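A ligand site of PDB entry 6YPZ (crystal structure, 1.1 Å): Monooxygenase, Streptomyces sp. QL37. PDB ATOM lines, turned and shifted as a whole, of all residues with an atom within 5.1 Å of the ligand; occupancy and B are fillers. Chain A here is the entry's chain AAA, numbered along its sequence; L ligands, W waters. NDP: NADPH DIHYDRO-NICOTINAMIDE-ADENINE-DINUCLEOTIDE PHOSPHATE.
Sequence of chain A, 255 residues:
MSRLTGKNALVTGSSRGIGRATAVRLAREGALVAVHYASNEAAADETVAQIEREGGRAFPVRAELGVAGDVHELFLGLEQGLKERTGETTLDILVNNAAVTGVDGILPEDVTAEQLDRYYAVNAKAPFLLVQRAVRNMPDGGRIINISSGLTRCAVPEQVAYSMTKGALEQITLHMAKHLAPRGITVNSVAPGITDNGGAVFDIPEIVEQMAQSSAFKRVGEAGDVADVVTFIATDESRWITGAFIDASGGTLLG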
ATOM      1  N   GLY A  13      24.599 -20.831  22.644  1.00  0.00           N
ATOM      2  CA  GLY A  13      23.670 -21.916  22.441  1.00  0.00           C
ATOM      3  C   GLY A  13      23.817 -22.571  21.084  1.00  0.00           C
ATOM      4  O   GLY A  13      22.843 -22.762  20.344  1.00  0.00           O
ATOM      5  N   SER A  14      25.061 -22.937  20.755  1.00  0.00           N
ATOM      6  CA  SER A  14      25.362 -23.594  19.458  1.00  0.00           C
ATOM      7  C   SER A  14      25.633 -25.075  19.574  1.00  0.00           C
ATOM      8  O   SER A  14      26.096 -25.685  18.592  1.00  0.00           O
ATOM      9  CB  SER A  14      26.402 -22.817  18.685  1.00  0.00           C
ATOM     10  OG  SER A  14      27.538 -22.488  19.488  1.00  0.00           O
ATOM     11  N   SER A  15      25.305 -25.678  20.697  1.00  0.00           N
ATOM     12  CA  SER A  15      25.276 -27.142  20.807  1.00  0.00           C
ATOM     13  C   SER A  15      24.237 -27.779  19.943  1.00  0.00           C
ATOM     14  O   SER A  15      24.408 -28.977  19.585  1.00  0.00           O
ATOM     15  CB  SER A  15      25.137 -27.549  22.251  1.00  0.00           C
ATOM     16  OG  SER A  15      23.991 -26.923  22.770  1.00  0.00           O
ATOM     17  N   ARG A  16      23.188 -27.082  19.599  1.00  0.00           N
ATOM     18  CA  ARG A  16      22.010 -27.710  18.998  1.00  0.00           C
ATOM     19  C   ARG A  16      21.253 -26.682  18.149  1.00  0.00           C
ATOM     20  O   ARG A  16      21.480 -25.480  18.310  1.00  0.00           O
ATOM     21  CB  ARG A  16      21.061 -28.185  20.146  1.00  0.00           C
ATOM     22  CG  ARG A  16      21.553 -29.235  21.108  1.00  0.00           C
ATOM     23  CD  ARG A  16      20.459 -29.384  22.145  1.00  0.00           C
ATOM     24  NE  ARG A  16      20.185 -28.542  23.269  1.00  0.00           N
ATOM     25  CZ  ARG A  16      19.009 -28.090  23.610  1.00  0.00           C
ATOM     26  NH1 ARG A  16      17.932 -28.329  22.839  1.00  0.00           N
ATOM     27  NH2 ARG A  16      18.813 -27.455  24.730  1.00  0.00           N
ATOM     28  N   GLY A  17      20.355 -27.139  17.309  1.00  0.00           N
ATOM     29  CA  GLY A  17      19.336 -26.271  16.711  1.00  0.00           C
ATOM     30  C   GLY A  17      19.892 -25.210  15.813  1.00  0.00           C
ATOM     31  O   GLY A  17      20.875 -25.448  15.077  1.00  0.00           O
ATOM     32  N   ILE A  18      19.243 -24.049  15.816  1.00  0.00           N
ATOM     33  CA  ILE A  18      19.655 -22.934  14.965  1.00  0.00           C
ATOM     34  C   ILE A  18      21.091 -22.533  15.269  1.00  0.00           C
ATOM     35  O   ILE A  18      21.851 -22.182  14.371  1.00  0.00           O
ATOM     36  CB  ILE A  18      18.698 -21.769  15.101  1.00  0.00           C
ATOM     37  CG1 ILE A  18      17.300 -22.149  14.630  1.00  0.00           C
ATOM     38  CG2 ILE A  18      19.205 -20.545  14.406  1.00  0.00           C
ATOM     39  CD1 ILE A  18      16.236 -21.146  14.976  1.00  0.00           C
ATOM     40  N   GLY A  19      21.458 -22.553  16.537  1.00  0.00           N
ATOM     41  CA  GLY A  19      22.814 -22.145  16.917  1.00  0.00           C
ATOM     42  C   GLY A  19      23.863 -23.083  16.324  1.00  0.00           C
ATOM     43  O   GLY A  19      24.898 -22.603  15.817  1.00  0.00           O
ATOM     44  N   HIS A  36      29.185 -22.302  22.250  1.00  0.00           N
ATOM     45  CA  HIS A  36      28.763 -22.157  23.645  1.00  0.00           C
ATOM     46  C   HIS A  36      27.536 -23.002  23.948  1.00  0.00           C
ATOM     47  O   HIS A  36      26.665 -23.220  23.081  1.00  0.00           O
ATOM     48  CB  HIS A  36      28.524 -20.680  23.963  1.00  0.00           C
ATOM     49  CG  HIS A  36      27.676 -20.455  25.138  1.00  0.00           C
ATOM     50  ND1 HIS A  36      26.329 -20.393  24.991  1.00  0.00           N
ATOM     51  CD2 HIS A  36      27.960 -20.510  26.448  1.00  0.00           C
ATOM     52  CE1 HIS A  36      25.827 -20.387  26.198  1.00  0.00           C
ATOM     53  NE2 HIS A  36      26.801 -20.414  27.130  1.00  0.00           N
ATOM     54  N   TYR A  37      27.501 -23.524  25.187  1.00  0.00           N
ATOM     55  CA  TYR A  37      26.403 -24.355  25.659  1.00  0.00           C
ATOM     56  C   TYR A  37      26.307 -24.222  27.164  1.00  0.00           C
ATOM     57  O   TYR A  37      27.207 -23.670  27.821  1.00  0.00           O
ATOM     58  CB  TYR A  37      26.633 -25.826  25.251  1.00  0.00           C
ATOM     59  CG  TYR A  37      27.778 -26.467  25.978  1.00  0.00           C
ATOM     60  CD1 TYR A  37      29.102 -26.239  25.666  1.00  0.00           C
ATOM     61  CD2 TYR A  37      27.489 -27.358  26.987  1.00  0.00           C
ATOM     62  CE1 TYR A  37      30.102 -26.844  26.387  1.00  0.00           C
ATOM     63  CE2 TYR A  37      28.502 -27.998  27.716  1.00  0.00           C
ATOM     64  CZ  TYR A  37      29.808 -27.724  27.428  1.00  0.00           C
ATOM     65  OH  TYR A  37      30.814 -28.376  28.105  1.00  0.00           O
ATOM     66  N   ALA A  38      25.267 -24.800  27.713  1.00  0.00           N
ATOM     67  CA  ALA A  38      25.057 -24.787  29.150  1.00  0.00           C
ATOM     68  C   ALA A  38      25.368 -26.114  29.735  1.00  0.00           C
ATOM     69  O   ALA A  38      26.110 -26.147  30.783  1.00  0.00           O
ATOM     70  CB  ALA A  38      23.628 -24.411  29.499  1.00  0.00           C
ATOM     71  N   SER A  39      24.753 -27.142  29.264  1.00  0.00           N
ATOM     72  CA  SER A  39      24.946 -28.465  29.862  1.00  0.00           C
ATOM     73  C   SER A  39      25.108 -29.588  28.877  1.00  0.00           C
ATOM     74  O   SER A  39      25.739 -30.612  29.307  1.00  0.00           O
ATOM     75  CB  SER A  39      23.867 -28.739  30.768  1.00  0.00           C
ATOM     76  OG  SER A  39      22.633 -28.779  30.176  1.00  0.00           O
ATOM     77  N   ASN A  40      24.625 -29.509  27.648  1.00  0.00           N
ATOM     78  CA  ASN A  40      24.703 -30.668  26.714  1.00  0.00           C
ATOM     79  C   ASN A  40      26.065 -30.637  26.066  1.00  0.00           C
ATOM     80  O   ASN A  40      26.239 -30.230  24.916  1.00  0.00           O
ATOM     81  CB  ASN A  40      23.586 -30.640  25.754  1.00  0.00           C
ATOM     82  CG  ASN A  40      23.417 -31.938  25.014  1.00  0.00           C
ATOM     83  OD1 ASN A  40      24.370 -32.708  24.914  1.00  0.00           O
ATOM     84  ND2 ASN A  40      22.221 -32.157  24.500  1.00  0.00           N
ATOM     85  N   ALA A  43      26.443 -32.604  22.776  1.00  0.00           N
ATOM     86  CA  ALA A  43      25.915 -31.901  21.609  1.00  0.00           C
ATOM     87  C   ALA A  43      26.911 -30.806  21.194  1.00  0.00           C
ATOM     88  O   ALA A  43      27.151 -30.628  19.997  1.00  0.00           O
ATOM     89  CB  ALA A  43      24.564 -31.315  21.891  1.00  0.00           C
ATOM     90  N   ALA A  63      28.920 -22.332  29.714  1.00  0.00           N
ATOM     91  CA  ALA A  63      28.522 -21.332  30.704  1.00  0.00           C
ATOM     92  C   ALA A  63      27.009 -21.322  30.784  1.00  0.00           C
ATOM     93  O   ALA A  63      26.334 -20.932  29.802  1.00  0.00           O
ATOM     94  CB  ALA A  63      29.057 -19.956  30.376  1.00  0.00           C
ATOM     95  N   GLU A  64      26.455 -21.633  31.909  1.00  0.00           N
ATOM     96  CA  GLU A  64      25.010 -21.444  32.210  1.00  0.00           C
ATOM     97  C   GLU A  64      24.732 -19.938  32.216  1.00  0.00           C
ATOM     98  O   GLU A  64      25.396 -19.235  32.993  1.00  0.00           O
ATOM     99  CB  GLU A  64      24.705 -22.012  33.599  1.00  0.00           C
ATOM    100  CG  GLU A  64      23.293 -21.791  34.137  1.00  0.00           C
ATOM    101  CD  GLU A  64      22.151 -22.530  33.458  1.00  0.00           C
ATOM    102  OE1 GLU A  64      22.397 -23.413  32.610  1.00  0.00           O
ATOM    103  OE2 GLU A  64      20.963 -22.259  33.772  1.00  0.00           O
ATOM    104  N   LEU A  65      23.846 -19.450  31.361  1.00  0.00           N
ATOM    105  CA  LEU A  65      23.425 -18.070  31.388  1.00  0.00           C
ATOM    106  C   LEU A  65      22.248 -17.927  32.365  1.00  0.00           C
ATOM    107  O   LEU A  65      21.473 -18.867  32.586  1.00  0.00           O
ATOM    108  CB  LEU A  65      23.020 -17.599  29.987  1.00  0.00           C
ATOM    109  CG  LEU A  65      24.162 -17.631  28.987  1.00  0.00           C
ATOM    110  CD1 LEU A  65      23.575 -17.274  27.626  1.00  0.00           C
ATOM    111  CD2 LEU A  65      25.298 -16.740  29.357  1.00  0.00           C
ATOM    112  N   ASN A  96      23.672 -13.696  19.732  1.00  0.00           N
ATOM    113  CA  ASN A  96      22.861 -14.015  20.932  1.00  0.00           C
ATOM    114  C   ASN A  96      21.748 -14.927  20.511  1.00  0.00           C
ATOM    115  O   ASN A  96      20.643 -14.478  20.142  1.00  0.00           O
ATOM    116  CB  ASN A  96      22.334 -12.740  21.566  1.00  0.00           C
ATOM    117  CG  ASN A  96      23.304 -12.008  22.425  1.00  0.00           C
ATOM    118  OD1 ASN A  96      23.427 -10.711  22.286  1.00  0.00           O
ATOM    119  ND2 ASN A  96      23.970 -12.630  23.295  1.00  0.00           N
ATOM    120  N   ASN A  97      21.991 -16.231  20.521  1.00  0.00           N
ATOM    121  CA  ASN A  97      21.100 -17.260  20.063  1.00  0.00           C
ATOM    122  C   ASN A  97      20.518 -18.105  21.190  1.00  0.00           C
ATOM    123  O   ASN A  97      19.350 -18.498  21.134  1.00  0.00           O
ATOM    124  CB  ASN A  97      21.839 -18.142  19.034  1.00  0.00           C
ATOM    125  CG  ASN A  97      21.049 -19.382  18.675  1.00  0.00           C
ATOM    126  OD1 ASN A  97      20.202 -19.345  17.761  1.00  0.00           O
ATOM    127  ND2 ASN A  97      21.337 -20.433  19.383  1.00  0.00           N
ATOM    128  N   ALA A  98      21.285 -18.373  22.249  1.00  0.00           N
ATOM    129  CA  ALA A  98      20.815 -19.228  23.341  1.00  0.00           C
ATOM    130  C   ALA A  98      19.563 -18.638  23.931  1.00  0.00           C
ATOM    131  O   ALA A  98      19.441 -17.402  24.114  1.00  0.00           O
ATOM    132  CB  ALA A  98      21.851 -19.306  24.453  1.00  0.00           C
ATOM    133  N   ALA A  99      18.637 -19.480  24.353  1.00  0.00           N
ATOM    134  CA  ALA A  99      17.423 -18.993  24.996  1.00  0.00           C
ATOM    135  C   ALA A  99      16.779 -20.134  25.740  1.00  0.00           C
ATOM    136  O   ALA A  99      16.955 -21.324  25.384  1.00  0.00           O
ATOM    137  CB  ALA A  99      16.413 -18.440  23.988  1.00  0.00           C
ATOM    138  N   VAL A 100      15.952 -19.787  26.706  1.00  0.00           N
ATOM    139  CA  VAL A 100      14.904 -20.632  27.302  1.00  0.00           C
ATOM    140  C   VAL A 100      13.769 -20.541  26.315  1.00  0.00           C
ATOM    141  O   VAL A 100      13.166 -19.475  26.072  1.00  0.00           O
ATOM    142  CB  VAL A 100      14.484 -20.100  28.681  1.00  0.00           C
ATOM    143  CG1 VAL A 100      13.368 -20.977  29.219  1.00  0.00           C
ATOM    144  CG2 VAL A 100      15.632 -20.062  29.630  1.00  0.00           C
ATOM    145  N   THR A 101      13.447 -21.652  25.654  1.00  0.00           N
ATOM    146  CA  THR A 101      12.628 -21.700  24.413  1.00  0.00           C
ATOM    147  C   THR A 101      12.013 -23.091  24.423  1.00  0.00           C
ATOM    148  O   THR A 101      12.745 -24.035  24.655  1.00  0.00           O
ATOM    149  CB  THR A 101      13.499 -21.273  23.196  1.00  0.00           C
ATOM    150  OG1 THR A 101      12.646 -21.154  22.049  1.00  0.00           O
ATOM    151  CG2 THR A 101      14.684 -22.184  23.007  1.00  0.00           C
ATOM    152  N   ARG A 118      13.192 -16.527  34.995  1.00  0.00           N
ATOM    153  CA  ARG A 118      14.141 -17.417  34.260  1.00  0.00           C
ATOM    154  C   ARG A 118      14.187 -16.969  32.794  1.00  0.00           C
ATOM    155  O   ARG A 118      15.281 -16.820  32.220  1.00  0.00           O
ATOM    156  CB  ARG A 118      13.732 -18.856  34.439  1.00  0.00           C
ATOM    157  CG  ARG A 118      14.587 -19.835  33.660  1.00  0.00           C
ATOM    158  CD  ARG A 118      16.035 -19.834  34.019  1.00  0.00           C
ATOM    159  NE  ARG A 118      16.722 -20.975  33.387  1.00  0.00           N
ATOM    160  CZ  ARG A 118      17.992 -21.173  33.497  1.00  0.00           C
ATOM    161  NH1 ARG A 118      18.769 -20.263  34.047  1.00  0.00           N
ATOM    162  NH2 ARG A 118      18.532 -22.246  32.901  1.00  0.00           N
ATOM    163  N   VAL A 122      17.766 -15.264  31.102  1.00  0.00           N
ATOM    164  CA  VAL A 122      18.494 -15.890  30.004  1.00  0.00           C
ATOM    165  C   VAL A 122      18.289 -15.152  28.689  1.00  0.00           C
ATOM    166  O   VAL A 122      19.245 -15.029  27.903  1.00  0.00           O
ATOM    167  CB  VAL A 122      18.083 -17.335  29.861  1.00  0.00           C
ATOM    168  CG1 VAL A 122      18.816 -18.027  28.697  1.00  0.00           C
ATOM    169  CG2 VAL A 122      18.330 -18.119  31.143  1.00  0.00           C
ATOM    170  N   ILE A 147      19.001 -13.143  18.069  1.00  0.00           N
ATOM    171  CA  ILE A 147      18.007 -14.056  17.515  1.00  0.00           C
ATOM    172  C   ILE A 147      16.714 -13.836  18.300  1.00  0.00           C
ATOM    173  O   ILE A 147      16.656 -14.156  19.485  1.00  0.00           O
ATOM    174  CB  ILE A 147      18.453 -15.508  17.543  1.00  0.00           C
ATOM    175  CG1 ILE A 147      19.822 -15.703  16.936  1.00  0.00           C
ATOM    176  CG2 ILE A 147      17.384 -16.354  16.860  1.00  0.00           C
ATOM    177  CD1 ILE A 147      19.975 -15.184  15.492  1.00  0.00           C
ATOM    178  N   SER A 148      15.714 -13.265  17.657  1.00  0.00           N
ATOM    179  CA  SER A 148      14.418 -12.960  18.259  1.00  0.00           C
ATOM    180  C   SER A 148      13.446 -14.057  17.911  1.00  0.00           C
ATOM    181  O   SER A 148      13.778 -15.262  17.995  1.00  0.00           O
ATOM    182  CB  SER A 148      14.014 -11.573  17.874  1.00  0.00           C
ATOM    183  OG  SER A 148      12.820 -11.256  18.604  1.00  0.00           O
ATOM    184  N   SER A 149      12.223 -13.679  17.568  1.00  0.00           N
ATOM    185  CA  SER A 149      11.168 -14.611  17.200  1.00  0.00           C
ATOM    186  C   SER A 149      10.087 -13.819  16.480  1.00  0.00           C
ATOM    187  O   SER A 149       9.780 -12.683  16.884  1.00  0.00           O
ATOM    188  CB  SER A 149      10.546 -15.207  18.457  1.00  0.00           C
ATOM    189  OG  SER A 149       9.366 -15.964  18.116  1.00  0.00           O
ATOM    190  N   GLY A 150       9.463 -14.426  15.493  1.00  0.00           N
ATOM    191  CA  GLY A 150       8.283 -13.838  14.900  1.00  0.00           C
ATOM    192  C   GLY A 150       7.134 -13.617  15.866  1.00  0.00           C
ATOM    193  O   GLY A 150       6.230 -12.826  15.549  1.00  0.00           O
ATOM    194  N   TYR A 162       7.692 -16.002  27.224  1.00  0.00           N
ATOM    195  CA  TYR A 162       8.820 -16.018  26.265  1.00  0.00           C
ATOM    196  C   TYR A 162       8.846 -14.745  25.405  1.00  0.00           C
ATOM    197  O   TYR A 162       9.875 -14.108  25.212  1.00  0.00           O
ATOM    198  CB  TYR A 162       8.653 -17.241  25.402  1.00  0.00           C
ATOM    199  CG  TYR A 162       9.501 -17.302  24.161  1.00  0.00           C
ATOM    200  CD1 TYR A 162      10.798 -17.787  24.207  1.00  0.00           C
ATOM    201  CD2 TYR A 162       9.018 -16.877  22.962  1.00  0.00           C
ATOM    202  CE1 TYR A 162      11.542 -17.897  23.046  1.00  0.00           C
ATOM    203  CE2 TYR A 162       9.745 -16.976  21.791  1.00  0.00           C
ATOM    204  CZ  TYR A 162      11.015 -17.503  21.831  1.00  0.00           C
ATOM    205  OH  TYR A 162      11.698 -17.669  20.661  1.00  0.00           O
ATOM    206  N   LYS A 166      11.649 -11.633  24.233  1.00  0.00           N
ATOM    207  CA  LYS A 166      12.071 -11.288  22.861  1.00  0.00           C
ATOM    208  C   LYS A 166      11.746  -9.855  22.546  1.00  0.00           C
ATOM    209  O   LYS A 166      12.496  -9.208  21.824  1.00  0.00           O
ATOM    210  CB  LYS A 166      11.465 -12.267  21.872  1.00  0.00           C
ATOM    211  CG  LYS A 166      11.925 -13.715  22.073  1.00  0.00           C
ATOM    212  CD  LYS A 166      13.413 -13.874  21.978  1.00  0.00           C
ATOM    213  CE  LYS A 166      13.832 -15.293  21.697  1.00  0.00           C
ATOM    214  NZ  LYS A 166      15.276 -15.429  21.551  1.00  0.00           N
ATOM    215  N   PRO A 192      13.244 -15.836  13.596  1.00  0.00           N
ATOM    216  CA  PRO A 192      12.744 -17.108  13.040  1.00  0.00           C
ATOM    217  C   PRO A 192      11.254 -17.261  13.228  1.00  0.00           C
ATOM    218  O   PRO A 192      10.643 -16.677  14.148  1.00  0.00           O
ATOM    219  CB  PRO A 192      13.505 -18.204  13.834  1.00  0.00           C
ATOM    220  CG  PRO A 192      14.626 -17.462  14.501  1.00  0.00           C
ATOM    221  CD  PRO A 192      14.044 -16.106  14.788  1.00  0.00           C
ATOM    222  N   GLY A 193      10.685 -18.129  12.412  1.00  0.00           N
ATOM    223  CA  GLY A 193       9.405 -18.729  12.663  1.00  0.00           C
ATOM    224  C   GLY A 193       9.617 -20.097  13.238  1.00  0.00           C
ATOM    225  O   GLY A 193      10.666 -20.392  13.819  1.00  0.00           O
ATOM    226  N   ILE A 194       8.616 -20.965  13.120  1.00  0.00           N
ATOM    227  CA  ILE A 194       8.765 -22.356  13.629  1.00  0.00           C
ATOM    228  C   ILE A 194       9.863 -23.036  12.841  1.00  0.00           C
ATOM    229  O   ILE A 194       9.814 -23.061  11.598  1.00  0.00           O
ATOM    230  CB  ILE A 194       7.463 -23.134  13.601  1.00  0.00           C
ATOM    231  CG1 ILE A 194       6.378 -22.452  14.400  1.00  0.00           C
ATOM    232  CG2 ILE A 194       7.652 -24.519  14.143  1.00  0.00           C
ATOM    233  CD1 ILE A 194       4.995 -23.099  14.239  1.00  0.00           C
ATOM    234  N   THR A 195      10.847 -23.558  13.548  1.00  0.00           N
ATOM    235  CA  THR A 195      12.077 -24.073  12.954  1.00  0.00           C
ATOM    236  C   THR A 195      12.426 -25.397  13.602  1.00  0.00           C
ATOM    237  O   THR A 195      12.514 -25.496  14.855  1.00  0.00           O
ATOM    238  CB  THR A 195      13.217 -23.068  13.163  1.00  0.00           C
ATOM    239  OG1 THR A 195      12.819 -21.763  12.722  1.00  0.00           O
ATOM    240  CG2 THR A 195      14.420 -23.443  12.368  1.00  0.00           C
ATOM    241  N   ASN A 197      14.449 -27.830  15.249  1.00  0.00           N
ATOM    242  CA  ASN A 197      15.665 -27.761  16.083  1.00  0.00           C
ATOM    243  C   ASN A 197      16.133 -29.158  16.500  1.00  0.00           C
ATOM    244  O   ASN A 197      17.023 -29.259  17.320  1.00  0.00           O
ATOM    245  CB  ASN A 197      15.470 -26.887  17.295  1.00  0.00           C
ATOM    246  CG  ASN A 197      14.390 -27.363  18.183  1.00  0.00           C
ATOM    247  OD1 ASN A 197      13.755 -28.384  17.953  1.00  0.00           O
ATOM    248  ND2 ASN A 197      13.935 -26.395  18.966  1.00  0.00           N
HETATM  249  PA  NDP L   1      17.242 -25.108  21.162  1.00  0.00           P
HETATM  250  O1A NDP L   1      16.282 -25.162  22.276  1.00  0.00           O
HETATM  251  O2A NDP L   1      17.283 -26.158  20.136  1.00  0.00           O
HETATM  252  O5B NDP L   1      18.717 -24.900  21.733  1.00  0.00           O
HETATM  253  C5B NDP L   1      18.915 -23.976  22.803  1.00  0.00           C
HETATM  254  C4B NDP L   1      20.359 -23.674  22.898  1.00  0.00           C
HETATM  255  O4B NDP L   1      20.536 -22.672  23.933  1.00  0.00           O
HETATM  256  C3B NDP L   1      21.238 -24.847  23.320  1.00  0.00           C
HETATM  257  O3B NDP L   1      22.548 -24.677  22.791  1.00  0.00           O
HETATM  258  C2B NDP L   1      21.264 -24.710  24.832  1.00  0.00           C
HETATM  259  O2B NDP L   1      22.356 -25.287  25.511  1.00  0.00           O
HETATM  260  C1B NDP L   1      21.307 -23.206  24.989  1.00  0.00           C
HETATM  261  N9A NDP L   1      20.768 -22.712  26.237  1.00  0.00           N
HETATM  262  C8A NDP L   1      19.507 -22.825  26.723  1.00  0.00           C
HETATM  263  N7A NDP L   1      19.335 -22.336  27.923  1.00  0.00           N
HETATM  264  C5A NDP L   1      20.592 -21.898  28.290  1.00  0.00           C
HETATM  265  C6A NDP L   1      21.104 -21.261  29.424  1.00  0.00           C
HETATM  266  N6A NDP L   1      20.402 -20.977  30.513  1.00  0.00           N
HETATM  267  N1A NDP L   1      22.391 -20.942  29.440  1.00  0.00           N
HETATM  268  C2A NDP L   1      23.114 -21.156  28.349  1.00  0.00           C
HETATM  269  N3A NDP L   1      22.753 -21.747  27.208  1.00  0.00           N
HETATM  270  C4A NDP L   1      21.468 -22.098  27.239  1.00  0.00           C
HETATM  271  O3  NDP L   1      16.983 -23.665  20.440  1.00  0.00           O
HETATM  272  PN  NDP L   1      16.514 -23.292  19.006  1.00  0.00           P
HETATM  273  O1N NDP L   1      17.592 -23.676  18.072  1.00  0.00           O
HETATM  274  O2N NDP L   1      15.150 -23.784  18.759  1.00  0.00           O
HETATM  275  O5D NDP L   1      16.387 -21.719  19.118  1.00  0.00           O
HETATM  276  C5D NDP L   1      17.557 -20.870  18.893  1.00  0.00           C
HETATM  277  C4D NDP L   1      17.084 -19.458  19.030  1.00  0.00           C
HETATM  278  O4D NDP L   1      16.055 -19.207  18.044  1.00  0.00           O
HETATM  279  C3D NDP L   1      16.503 -19.044  20.369  1.00  0.00           C
HETATM  280  O3D NDP L   1      16.760 -17.670  20.638  1.00  0.00           O
HETATM  281  C2D NDP L   1      15.022 -19.205  20.114  1.00  0.00           C
HETATM  282  O2D NDP L   1      14.216 -18.444  21.027  1.00  0.00           O
HETATM  283  C1D NDP L   1      14.897 -18.726  18.720  1.00  0.00           C
HETATM  284  N1N NDP L   1      13.722 -19.187  18.015  1.00  0.00           N
HETATM  285  C2N NDP L   1      13.517 -20.520  17.733  1.00  0.00           C
HETATM  286  C3N NDP L   1      12.377 -20.981  17.129  1.00  0.00           C
HETATM  287  C7N NDP L   1      12.171 -22.388  16.770  1.00  0.00           C
HETATM  288  O7N NDP L   1      13.109 -23.272  16.880  1.00  0.00           O
HETATM  289  N7N NDP L   1      11.041 -22.688  16.263  1.00  0.00           N
HETATM  290  C4N NDP L   1      11.359 -20.037  16.769  1.00  0.00           C
HETATM  291  C5N NDP L   1      11.636 -18.687  17.027  1.00  0.00           C
HETATM  292  C6N NDP L   1      12.760 -18.286  17.614  1.00  0.00           C
HETATM  293  P2B NDP L   1      22.334 -26.865  25.913  1.00  0.00           P
HETATM  294  O1X NDP L   1      21.028 -27.120  26.615  1.00  0.00           O
HETATM  295  O2X NDP L   1      22.424 -27.661  24.620  1.00  0.00           O
HETATM  296  O3X NDP L   1      23.536 -26.999  26.799  1.00  0.00           O
HETATM  297  O   HOH W   1      20.456 -26.379  29.100  1.00  0.00           O
HETATM  298  O   HOH W   2      12.900 -23.431  20.303  1.00  0.00           O
HETATM  299  O   HOH W   3       8.060 -19.320  17.014  1.00  0.00           O
HETATM  300  O   HOH W   4      13.528 -25.564  22.163  1.00  0.00           O
HETATM  301  O   HOH W   5      20.125 -29.637  27.121  1.00  0.00           O
HETATM  302  O   HOH W   6      20.082 -23.072  18.992  1.00  0.00           O
HETATM  303  O   HOH W   7      17.511 -28.689  19.935  1.00  0.00           O
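N6A of the ligand lies close to NH2 of Arg 118.
N of Ser 14 touches O3B of the ligand, 3.7 Å away.
CA of Gly 17 touches O1N of the ligand, at 3.4 Å.
His 36 touches the ligand.
Tyr 37 touches the ligand (CB to O3X, 3.7 Å).
O of Ala 63 touches C2A of the ligand (3.5 Å).
Glu 64 touches the ligand.
Ala 98 touches the ligand (CA to O4B, 3.5 Å).
Ala 99 touches the ligand.
Val 122 touches the ligand.
Ile 147 touches the ligand (CG2 to O4D, 3.4 Å).
Ser 148 touches the ligand (O to C6N, 3.2 Å).
Ser 149 touches the ligand.
O of Pro 192 touches C5N of the ligand, 3.6 Å away.
Ile 194 touches the ligand (CA to N7N, 3.5 Å).
Hydrophobic or aromatic side chains within 4 Å of the ligand: Ile 18, His 36, Tyr 37, Ala 38, Leu 65, Ala 98, Ala 99, Val 122, Ile 147, Tyr 162 and Pro 192.
Within 4 Å of the ligand: Gly 13, Ser 14, Ser 15, Arg 16, Gly 17, Ile 18, His 36, Tyr 37, Ala 38, Ser 39, Asn 40, Ala 63, Glu 64, Leu 65, Asn 97, Ala 98, Ala 99, Thr 101, Arg 118, Val 122, Ile 147, Ser 148, Ser 149, Tyr 162, Lys 166, Pro 192, Gly 193, Ile 194, Thr 195 and Asn 197.
The nearest printed residue that does not touch the ligand is Gly 19 (4.3 Å).
Water W7 lies within hydrogen-bond range of O2A of the ligand, O of Asn 197 and NH1 of Arg 16.
Water W1 bridges O1X of the ligand and OG of Ser 39.
Water W5 bridges an oxygen (O1X) of the ligand (2.7 Å) and the guanidinium group of Arg 16 (3.5 Å).
Water W2 lies within hydrogen-bond range of an oxygen (O2N) of the ligand, the side-chain hydroxyl (OG1) of Thr 101 and the side-chain amide nitrogen (ND2) of Asn 197.
Water W4 lies within hydrogen-bond range of O1A of the ligand (2.8 Å), O of Thr 101 (3.0 Å) and ND2 of Asn 197 (3.3 Å).
O2X of the ligand sits at hydrogen-bond distance from OG of Ser 15 (2.5 Å).
The side-chain hydroxyl of Tyr 162 is in hydrogen-bond range of an oxygen (O2D) of the ligand (2.7 Å).
O3X of the ligand is in hydrogen-bond range of N of Ser 39, 2.8 Å away.
NE of Arg 16 lies within salt-bridge range of O2X of the ligand (2.8 Å).
O of Asn 97 lies within hydrogen-bond range of O3D of the ligand (2.8 Å).
An oxygen (O1N) of the ligand sits at hydrogen-bond distance from the backbone NH (N) of Ile 18 (2.8 Å).
N of Leu 65 lies within hydrogen-bond range of N1A of the ligand (2.8 Å).
The backbone carbonyl oxygen (O) of Leu 65 is in hydrogen-bond range of a nitrogen (N6A) of the ligand, 3.1 Å away.
NZ of Lys 166 lies within hydrogen-bond range of O3D of the ligand (2.8 Å).
N7N of the ligand sits at hydrogen-bond distance from O of Thr 195 (3.5 Å).
O3X of the ligand sits at hydrogen-bond distance from N of Asn 40, at 2.9 Å.
An oxygen (O2N) of the ligand is in hydrogen-bond range of the side-chain amide nitrogen of Asn 197 (2.9 Å).
N of Ala 38 sits at hydrogen-bond distance from O3X of the ligand, 2.9 Å away.
The backbone carbonyl oxygen (O) of Gly 13 sits close to an oxygen (O3B) of the ligand.
O of Gly 193 lies close to N7N of the ligand (3.4 Å).
An oxygen (O2D) of the ligand lies within hydrogen-bond range of the side-chain hydroxyl (OG1) of Thr 101 (3.3 Å).
O of Leu 65 is in hydrogen-bond range of NH1 of Arg 118.
The side-chain hydroxyl (OG1) of Thr 195 lies within hydrogen-bond range of the backbone carbonyl oxygen (O) of Gly 193, 2.8 Å away.
The side-chain amide oxygen (OD1) of Asn 40 lies within hydrogen-bond range of the backbone NH (N) of Ala 43 (3.0 Å).
The backbone NH (N) of Gly 13 sits at hydrogen-bond distance from a ring nitrogen (ND1) of His 36, at 2.9 Å.
N of Ile 147 lies within hydrogen-bond range of O of Asn 96 (3.0 Å).
N of Ser 14 lies within hydrogen-bond range of O of His 36 (2.8 Å).
O of Tyr 37 lies within hydrogen-bond range of N of Ala 63.
The backbone carbonyl oxygen of Pro 192 lies within hydrogen-bond range of the backbone NH of Gly 150.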
